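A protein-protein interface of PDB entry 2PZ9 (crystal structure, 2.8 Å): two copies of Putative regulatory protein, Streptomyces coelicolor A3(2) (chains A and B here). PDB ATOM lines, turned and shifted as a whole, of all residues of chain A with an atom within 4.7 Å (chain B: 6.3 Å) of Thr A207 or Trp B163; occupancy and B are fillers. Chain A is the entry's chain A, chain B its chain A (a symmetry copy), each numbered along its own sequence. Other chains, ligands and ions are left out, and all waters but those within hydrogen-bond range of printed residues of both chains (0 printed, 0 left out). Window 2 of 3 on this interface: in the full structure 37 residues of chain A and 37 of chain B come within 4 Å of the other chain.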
ATOM      1  N   ALA A 203      17.231 -13.450   5.494  1.00  0.00           N
ATOM      2  CA  ALA A 203      15.795 -13.224   5.289  1.00  0.00           C
ATOM      3  C   ALA A 203      15.021 -14.546   5.142  1.00  0.00           C
ATOM      4  O   ALA A 203      13.999 -14.760   5.797  1.00  0.00           O
ATOM      5  CB  ALA A 203      15.564 -12.336   4.116  1.00  0.00           C
ATOM      6  N   ALA A 204      15.568 -15.436   4.312  1.00  0.00           N
ATOM      7  CA  ALA A 204      14.951 -16.700   3.998  1.00  0.00           C
ATOM      8  C   ALA A 204      14.784 -17.419   5.311  1.00  0.00           C
ATOM      9  O   ALA A 204      13.702 -17.865   5.663  1.00  0.00           O
ATOM     10  CB  ALA A 204      15.840 -17.506   3.045  1.00  0.00           C
ATOM     11  N   LEU A 205      15.867 -17.484   6.055  1.00  0.00           N
ATOM     12  CA  LEU A 205      15.888 -18.268   7.255  1.00  0.00           C
ATOM     13  C   LEU A 205      14.863 -17.752   8.276  1.00  0.00           C
ATOM     14  O   LEU A 205      14.121 -18.532   8.885  1.00  0.00           O
ATOM     15  CB  LEU A 205      17.288 -18.229   7.821  1.00  0.00           C
ATOM     16  CG  LEU A 205      17.357 -18.299   9.326  1.00  0.00           C
ATOM     17  CD1 LEU A 205      16.692 -19.551   9.894  1.00  0.00           C
ATOM     18  CD2 LEU A 205      18.823 -18.294   9.652  1.00  0.00           C
ATOM     19  N   VAL A 206      14.826 -16.433   8.444  1.00  0.00           N
ATOM     20  CA  VAL A 206      13.921 -15.837   9.373  1.00  0.00           C
ATOM     21  C   VAL A 206      12.485 -16.054   8.897  1.00  0.00           C
ATOM     22  O   VAL A 206      11.570 -16.321   9.711  1.00  0.00           O
ATOM     23  CB  VAL A 206      14.246 -14.376   9.567  1.00  0.00           C
ATOM     24  CG1 VAL A 206      13.108 -13.673  10.271  1.00  0.00           C
ATOM     25  CG2 VAL A 206      15.513 -14.248  10.369  1.00  0.00           C
ATOM     26  N   THR A 207      12.288 -15.978   7.582  1.00  0.00           N
ATOM     27  CA  THR A 207      10.973 -16.141   6.990  1.00  0.00           C
ATOM     28  C   THR A 207      10.525 -17.559   7.205  1.00  0.00           C
ATOM     29  O   THR A 207       9.378 -17.798   7.553  1.00  0.00           O
ATOM     30  CB  THR A 207      11.005 -15.812   5.502  1.00  0.00           C
ATOM     31  OG1 THR A 207      11.373 -14.435   5.341  1.00  0.00           O
ATOM     32  CG2 THR A 207       9.650 -16.045   4.861  1.00  0.00           C
ATOM     33  N   ALA A 208      11.441 -18.503   7.037  1.00  0.00           N
ATOM     34  CA  ALA A 208      11.132 -19.905   7.241  1.00  0.00           C
ATOM     35  C   ALA A 208      10.672 -20.181   8.676  1.00  0.00           C
ATOM     36  O   ALA A 208       9.756 -20.991   8.914  1.00  0.00           O
ATOM     37  CB  ALA A 208      12.330 -20.768   6.881  1.00  0.00           C
ATOM     38  N   VAL A 209      11.307 -19.518   9.633  1.00  0.00           N
ATOM     39  CA  VAL A 209      11.003 -19.767  11.030  1.00  0.00           C
ATOM     40  C   VAL A 209       9.676 -19.112  11.332  1.00  0.00           C
ATOM     41  O   VAL A 209       8.856 -19.675  12.080  1.00  0.00           O
ATOM     42  CB  VAL A 209      12.116 -19.281  11.985  1.00  0.00           C
ATOM     43  CG1 VAL A 209      11.709 -19.452  13.451  1.00  0.00           C
ATOM     44  CG2 VAL A 209      13.392 -20.045  11.726  1.00  0.00           C
ATOM     45  N   GLU A 210       9.458 -17.939  10.725  1.00  0.00           N
ATOM     46  CA  GLU A 210       8.142 -17.324  10.750  1.00  0.00           C
ATOM     47  C   GLU A 210       7.072 -18.300  10.245  1.00  0.00           C
ATOM     48  O   GLU A 210       6.005 -18.411  10.857  1.00  0.00           O
ATOM     49  CB  GLU A 210       8.109 -16.017   9.969  1.00  0.00           C
ATOM     50  CG  GLU A 210       6.681 -15.489   9.652  1.00  0.00           C
ATOM     51  CD  GLU A 210       5.808 -15.179  10.905  1.00  0.00           C
ATOM     52  OE1 GLU A 210       6.359 -14.792  11.976  1.00  0.00           O
ATOM     53  OE2 GLU A 210       4.554 -15.309  10.815  1.00  0.00           O
ATOM     54  N   HIS A 211       7.346 -19.028   9.165  1.00  0.00           N
ATOM     55  CA  HIS A 211       6.356 -19.987   8.677  1.00  0.00           C
ATOM     56  C   HIS A 211       6.092 -21.109   9.653  1.00  0.00           C
ATOM     57  O   HIS A 211       4.958 -21.490   9.835  1.00  0.00           O
ATOM     58  CB  HIS A 211       6.698 -20.517   7.292  1.00  0.00           C
ATOM     59  CG  HIS A 211       6.405 -19.539   6.204  1.00  0.00           C
ATOM     60  ND1 HIS A 211       7.351 -18.662   5.712  1.00  0.00           N
ATOM     61  CD2 HIS A 211       5.259 -19.262   5.543  1.00  0.00           C
ATOM     62  CE1 HIS A 211       6.807 -17.907   4.778  1.00  0.00           C
ATOM     63  NE2 HIS A 211       5.539 -18.251   4.657  1.00  0.00           N
ATOM     64  N   GLN B 154       8.452 -24.371  -8.990  1.00  0.00           N
ATOM     65  CA  GLN B 154       7.998 -22.993  -8.859  1.00  0.00           C
ATOM     66  C   GLN B 154       7.265 -22.561 -10.105  1.00  0.00           C
ATOM     67  O   GLN B 154       6.163 -22.020 -10.001  1.00  0.00           O
ATOM     68  CB  GLN B 154       9.166 -22.063  -8.560  1.00  0.00           C
ATOM     69  CG  GLN B 154       9.706 -22.292  -7.162  1.00  0.00           C
ATOM     70  CD  GLN B 154      10.810 -21.335  -6.757  1.00  0.00           C
ATOM     71  OE1 GLN B 154      11.853 -21.263  -7.404  1.00  0.00           O
ATOM     72  NE2 GLN B 154      10.600 -20.618  -5.654  1.00  0.00           N
ATOM     73  N   LEU B 159       5.346 -24.429  -5.615  1.00  0.00           N
ATOM     74  CA  LEU B 159       6.227 -23.982  -4.549  1.00  0.00           C
ATOM     75  C   LEU B 159       6.332 -22.461  -4.722  1.00  0.00           C
ATOM     76  O   LEU B 159       6.688 -21.971  -5.791  1.00  0.00           O
ATOM     77  CB  LEU B 159       7.586 -24.680  -4.682  1.00  0.00           C
ATOM     78  CG  LEU B 159       8.854 -24.189  -3.993  1.00  0.00           C
ATOM     79  CD1 LEU B 159       8.937 -24.661  -2.576  1.00  0.00           C
ATOM     80  CD2 LEU B 159      10.017 -24.719  -4.752  1.00  0.00           C
ATOM     81  N   ASP B 160       5.971 -21.725  -3.683  1.00  0.00           N
ATOM     82  CA  ASP B 160       5.962 -20.277  -3.711  1.00  0.00           C
ATOM     83  C   ASP B 160       7.145 -19.701  -4.518  1.00  0.00           C
ATOM     84  O   ASP B 160       8.303 -19.984  -4.198  1.00  0.00           O
ATOM     85  CB  ASP B 160       6.012 -19.804  -2.270  1.00  0.00           C
ATOM     86  CG  ASP B 160       5.597 -18.374  -2.103  1.00  0.00           C
ATOM     87  OD1 ASP B 160       5.920 -17.533  -2.984  1.00  0.00           O
ATOM     88  OD2 ASP B 160       4.960 -18.098  -1.058  1.00  0.00           O
ATOM     89  N   PRO B 161       6.857 -18.886  -5.563  1.00  0.00           N
ATOM     90  CA  PRO B 161       7.935 -18.443  -6.464  1.00  0.00           C
ATOM     91  C   PRO B 161       8.877 -17.427  -5.817  1.00  0.00           C
ATOM     92  O   PRO B 161       9.907 -17.080  -6.404  1.00  0.00           O
ATOM     93  CB  PRO B 161       7.175 -17.813  -7.644  1.00  0.00           C
ATOM     94  CG  PRO B 161       5.910 -17.335  -7.054  1.00  0.00           C
ATOM     95  CD  PRO B 161       5.550 -18.328  -5.968  1.00  0.00           C
ATOM     96  N   ALA B 162       8.509 -16.968  -4.621  1.00  0.00           N
ATOM     97  CA  ALA B 162       9.294 -16.008  -3.862  1.00  0.00           C
ATOM     98  C   ALA B 162      10.568 -16.609  -3.271  1.00  0.00           C
ATOM     99  O   ALA B 162      11.530 -15.903  -3.136  1.00  0.00           O
ATOM    100  CB  ALA B 162       8.438 -15.374  -2.778  1.00  0.00           C
ATOM    101  N   TRP B 163      10.584 -17.898  -2.924  1.00  0.00           N
ATOM    102  CA  TRP B 163      11.778 -18.545  -2.341  1.00  0.00           C
ATOM    103  C   TRP B 163      12.915 -18.682  -3.328  1.00  0.00           C
ATOM    104  O   TRP B 163      12.700 -18.968  -4.496  1.00  0.00           O
ATOM    105  CB  TRP B 163      11.484 -19.967  -1.873  1.00  0.00           C
ATOM    106  CG  TRP B 163      10.537 -20.084  -0.766  1.00  0.00           C
ATOM    107  CD1 TRP B 163       9.231 -20.445  -0.855  1.00  0.00           C
ATOM    108  CD2 TRP B 163      10.800 -19.851   0.620  1.00  0.00           C
ATOM    109  NE1 TRP B 163       8.648 -20.446   0.393  1.00  0.00           N
ATOM    110  CE2 TRP B 163       9.588 -20.092   1.322  1.00  0.00           C
ATOM    111  CE3 TRP B 163      11.937 -19.462   1.342  1.00  0.00           C
ATOM    112  CZ2 TRP B 163       9.480 -19.959   2.717  1.00  0.00           C
ATOM    113  CZ3 TRP B 163      11.832 -19.328   2.726  1.00  0.00           C
ATOM    114  CH2 TRP B 163      10.605 -19.572   3.402  1.00  0.00           C
ATOM    115  N   ASP B 164      14.138 -18.535  -2.856  1.00  0.00           N
ATOM    116  CA  ASP B 164      15.240 -18.964  -3.678  1.00  0.00           C
ATOM    117  C   ASP B 164      15.433 -20.463  -3.485  1.00  0.00           C
ATOM    118  O   ASP B 164      15.608 -20.942  -2.371  1.00  0.00           O
ATOM    119  CB  ASP B 164      16.522 -18.226  -3.345  1.00  0.00           C
ATOM    120  CG  ASP B 164      17.520 -18.256  -4.480  1.00  0.00           C
ATOM    121  OD1 ASP B 164      17.937 -19.356  -4.926  1.00  0.00           O
ATOM    122  OD2 ASP B 164      17.885 -17.148  -4.916  1.00  0.00           O
ATOM    123  N   PRO B 165      15.397 -21.209  -4.595  1.00  0.00           N
ATOM    124  CA  PRO B 165      15.683 -22.626  -4.587  1.00  0.00           C
ATOM    125  C   PRO B 165      16.857 -22.940  -3.660  1.00  0.00           C
ATOM    126  O   PRO B 165      16.758 -23.824  -2.808  1.00  0.00           O
ATOM    127  CB  PRO B 165      16.069 -22.878  -6.042  1.00  0.00           C
ATOM    128  CG  PRO B 165      15.193 -21.970  -6.779  1.00  0.00           C
ATOM    129  CD  PRO B 165      15.073 -20.732  -5.951  1.00  0.00           C
ATOM    130  N   VAL B 166      17.950 -22.198  -3.847  1.00  0.00           N
ATOM    131  CA  VAL B 166      19.155 -22.307  -3.038  1.00  0.00           C
ATOM    132  C   VAL B 166      18.813 -22.365  -1.542  1.00  0.00           C
ATOM    133  O   VAL B 166      19.293 -23.243  -0.826  1.00  0.00           O
ATOM    134  CB  VAL B 166      20.156 -21.151  -3.384  1.00  0.00           C
ATOM    135  CG1 VAL B 166      21.314 -21.096  -2.426  1.00  0.00           C
ATOM    136  CG2 VAL B 166      20.702 -21.340  -4.778  1.00  0.00           C
ATOM    137  N   ASP B 167      17.973 -21.448  -1.081  1.00  0.00           N
ATOM    138  CA  ASP B 167      17.578 -21.437   0.326  1.00  0.00           C
ATOM    139  C   ASP B 167      16.706 -22.659   0.689  1.00  0.00           C
ATOM    140  O   ASP B 167      16.876 -23.259   1.766  1.00  0.00           O
ATOM    141  CB  ASP B 167      16.882 -20.114   0.700  1.00  0.00           C
ATOM    142  CG  ASP B 167      17.817 -18.889   0.579  1.00  0.00           C
ATOM    143  OD1 ASP B 167      18.886 -18.870   1.239  1.00  0.00           O
ATOM    144  OD2 ASP B 167      17.480 -17.927  -0.164  1.00  0.00           O
ATOM    145  N   VAL B 168      15.792 -23.032  -0.207  1.00  0.00           N
ATOM    146  CA  VAL B 168      14.854 -24.129   0.029  1.00  0.00           C
ATOM    147  C   VAL B 168      15.611 -25.444   0.249  1.00  0.00           C
ATOM    148  O   VAL B 168      15.381 -26.159   1.237  1.00  0.00           O
ATOM    149  CB  VAL B 168      13.838 -24.265  -1.151  1.00  0.00           C
ATOM    150  CG1 VAL B 168      12.876 -25.409  -0.911  1.00  0.00           C
ATOM    151  CG2 VAL B 168      13.089 -22.972  -1.367  1.00  0.00           C
ATOM    152  N   LEU B 171      18.029 -25.312   3.587  1.00  0.00           N
ATOM    153  CA  LEU B 171      17.160 -25.384   4.756  1.00  0.00           C
ATOM    154  C   LEU B 171      16.627 -26.789   5.029  1.00  0.00           C
ATOM    155  O   LEU B 171      16.817 -27.348   6.120  1.00  0.00           O
ATOM    156  CB  LEU B 171      15.974 -24.421   4.618  1.00  0.00           C
ATOM    157  CG  LEU B 171      16.351 -22.931   4.650  1.00  0.00           C
ATOM    158  CD1 LEU B 171      15.242 -22.068   4.037  1.00  0.00           C
ATOM    159  CD2 LEU B 171      16.768 -22.452   6.066  1.00  0.00           C
ATOM    160  N   MET B 212       6.708 -24.589   6.544  1.00  0.00           N
ATOM    161  CA  MET B 212       7.479 -23.733   5.652  1.00  0.00           C
ATOM    162  C   MET B 212       6.975 -23.683   4.222  1.00  0.00           C
ATOM    163  O   MET B 212       6.683 -22.607   3.699  1.00  0.00           O
ATOM    164  CB  MET B 212       8.899 -24.177   5.618  1.00  0.00           C
ATOM    165  CG  MET B 212       9.701 -23.522   6.644  1.00  0.00           C
ATOM    166  SD  MET B 212      11.179 -24.733   6.901  1.00  0.00           S
ATOM    167  CE  MET B 212      12.271 -24.414   5.290  1.00  0.00           C
ATOM    168  N   PHE B 213       6.897 -24.850   3.591  1.00  0.00           N
ATOM    169  CA  PHE B 213       6.431 -24.956   2.211  1.00  0.00           C
ATOM    170  C   PHE B 213       5.198 -25.859   2.145  1.00  0.00           C
ATOM    171  O   PHE B 213       5.340 -27.075   1.959  1.00  0.00           O
ATOM    172  CB  PHE B 213       7.535 -25.514   1.309  1.00  0.00           C
ATOM    173  CG  PHE B 213       8.920 -25.079   1.692  1.00  0.00           C
ATOM    174  CD1 PHE B 213       9.714 -25.879   2.517  1.00  0.00           C
ATOM    175  CD2 PHE B 213       9.446 -23.888   1.213  1.00  0.00           C
ATOM    176  CE1 PHE B 213      11.005 -25.478   2.860  1.00  0.00           C
ATOM    177  CE2 PHE B 213      10.733 -23.489   1.558  1.00  0.00           C
ATOM    178  CZ  PHE B 213      11.509 -24.280   2.375  1.00  0.00           C
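The backbone carbonyl oxygen (O) of Thr A207 is in hydrogen-bond range of a ring nitrogen (ND1) of His A211. The backbone carbonyl oxygen (O) of Ala A203 is in hydrogen-bond range of the side-chain hydroxyl (OG1) of Thr A207 (2.7 Å). The side-chain amide nitrogen (NE2) of Gln B154 sits at hydrogen-bond distance from the backbone carbonyl oxygen (O) of Trp B163, at 2.9 Å.
Among the printed residues, pairs that only touch across the chains: Ala A208 with Met B212 (3.4 Å), Ala A204 with Asp B167 (3.4 Å), His A211 with Met B212 (3.7 Å), Ala A204 with Trp B163 (3.8 Å), Ala A208 with Trp B163 (3.9 Å), His A211 with Trp B163 (3.9 Å) and Thr A207 with Trp B163 (3.9 Å).
Printed residues of chain B within 4 Å of Ala A204: Trp B163 (3.8 Å) and Asp B167 (3.4 Å). Leu A205 touches none of the printed residues of chain B. Thr A207 touches just one residue of chain B: Trp B163 (3.9 Å). Of the printed residues of chain B, Ala A208 touches Trp B163 (3.9 Å) and Met B212 (3.4 Å). Leu B159 touches none of the printed residues of chain A. Printed residues of chain A within 4 Å of Trp B163: Ala A204, Thr A207, Ala A208 and His A211. Of the printed residues of chain A, Asp B167 touches Ala A204 (3.4 Å). Printed residues of chain A within 4 Å of Met B212: Ala A208 and His A211. The nearest residue of chain B that does not touch Thr A207 is Met B212 (5.8 Å).
Of the 9 printed residues of chain A, 4 touch a printed residue of chain B. Of the 14 printed residues of chain B, 3 touch a printed residue of chain A. Printed residues of chain B that touch a printed residue of chain A: Trp B163, Asp B167 and Met B212. Hydrophobic or aromatic side chains of chain B within 4 Å of the printed part of chain A: Trp B163 and Met B212. Among the printed residues, no Asp or Glu carboxylate lies within 4 Å of a Lys or Arg side-chain nitrogen of the other chain.
No position is printed for both chains. Of the 7 pairs that touch across the chains among the printed residues, none has its exchanged pair printed and touching as well.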
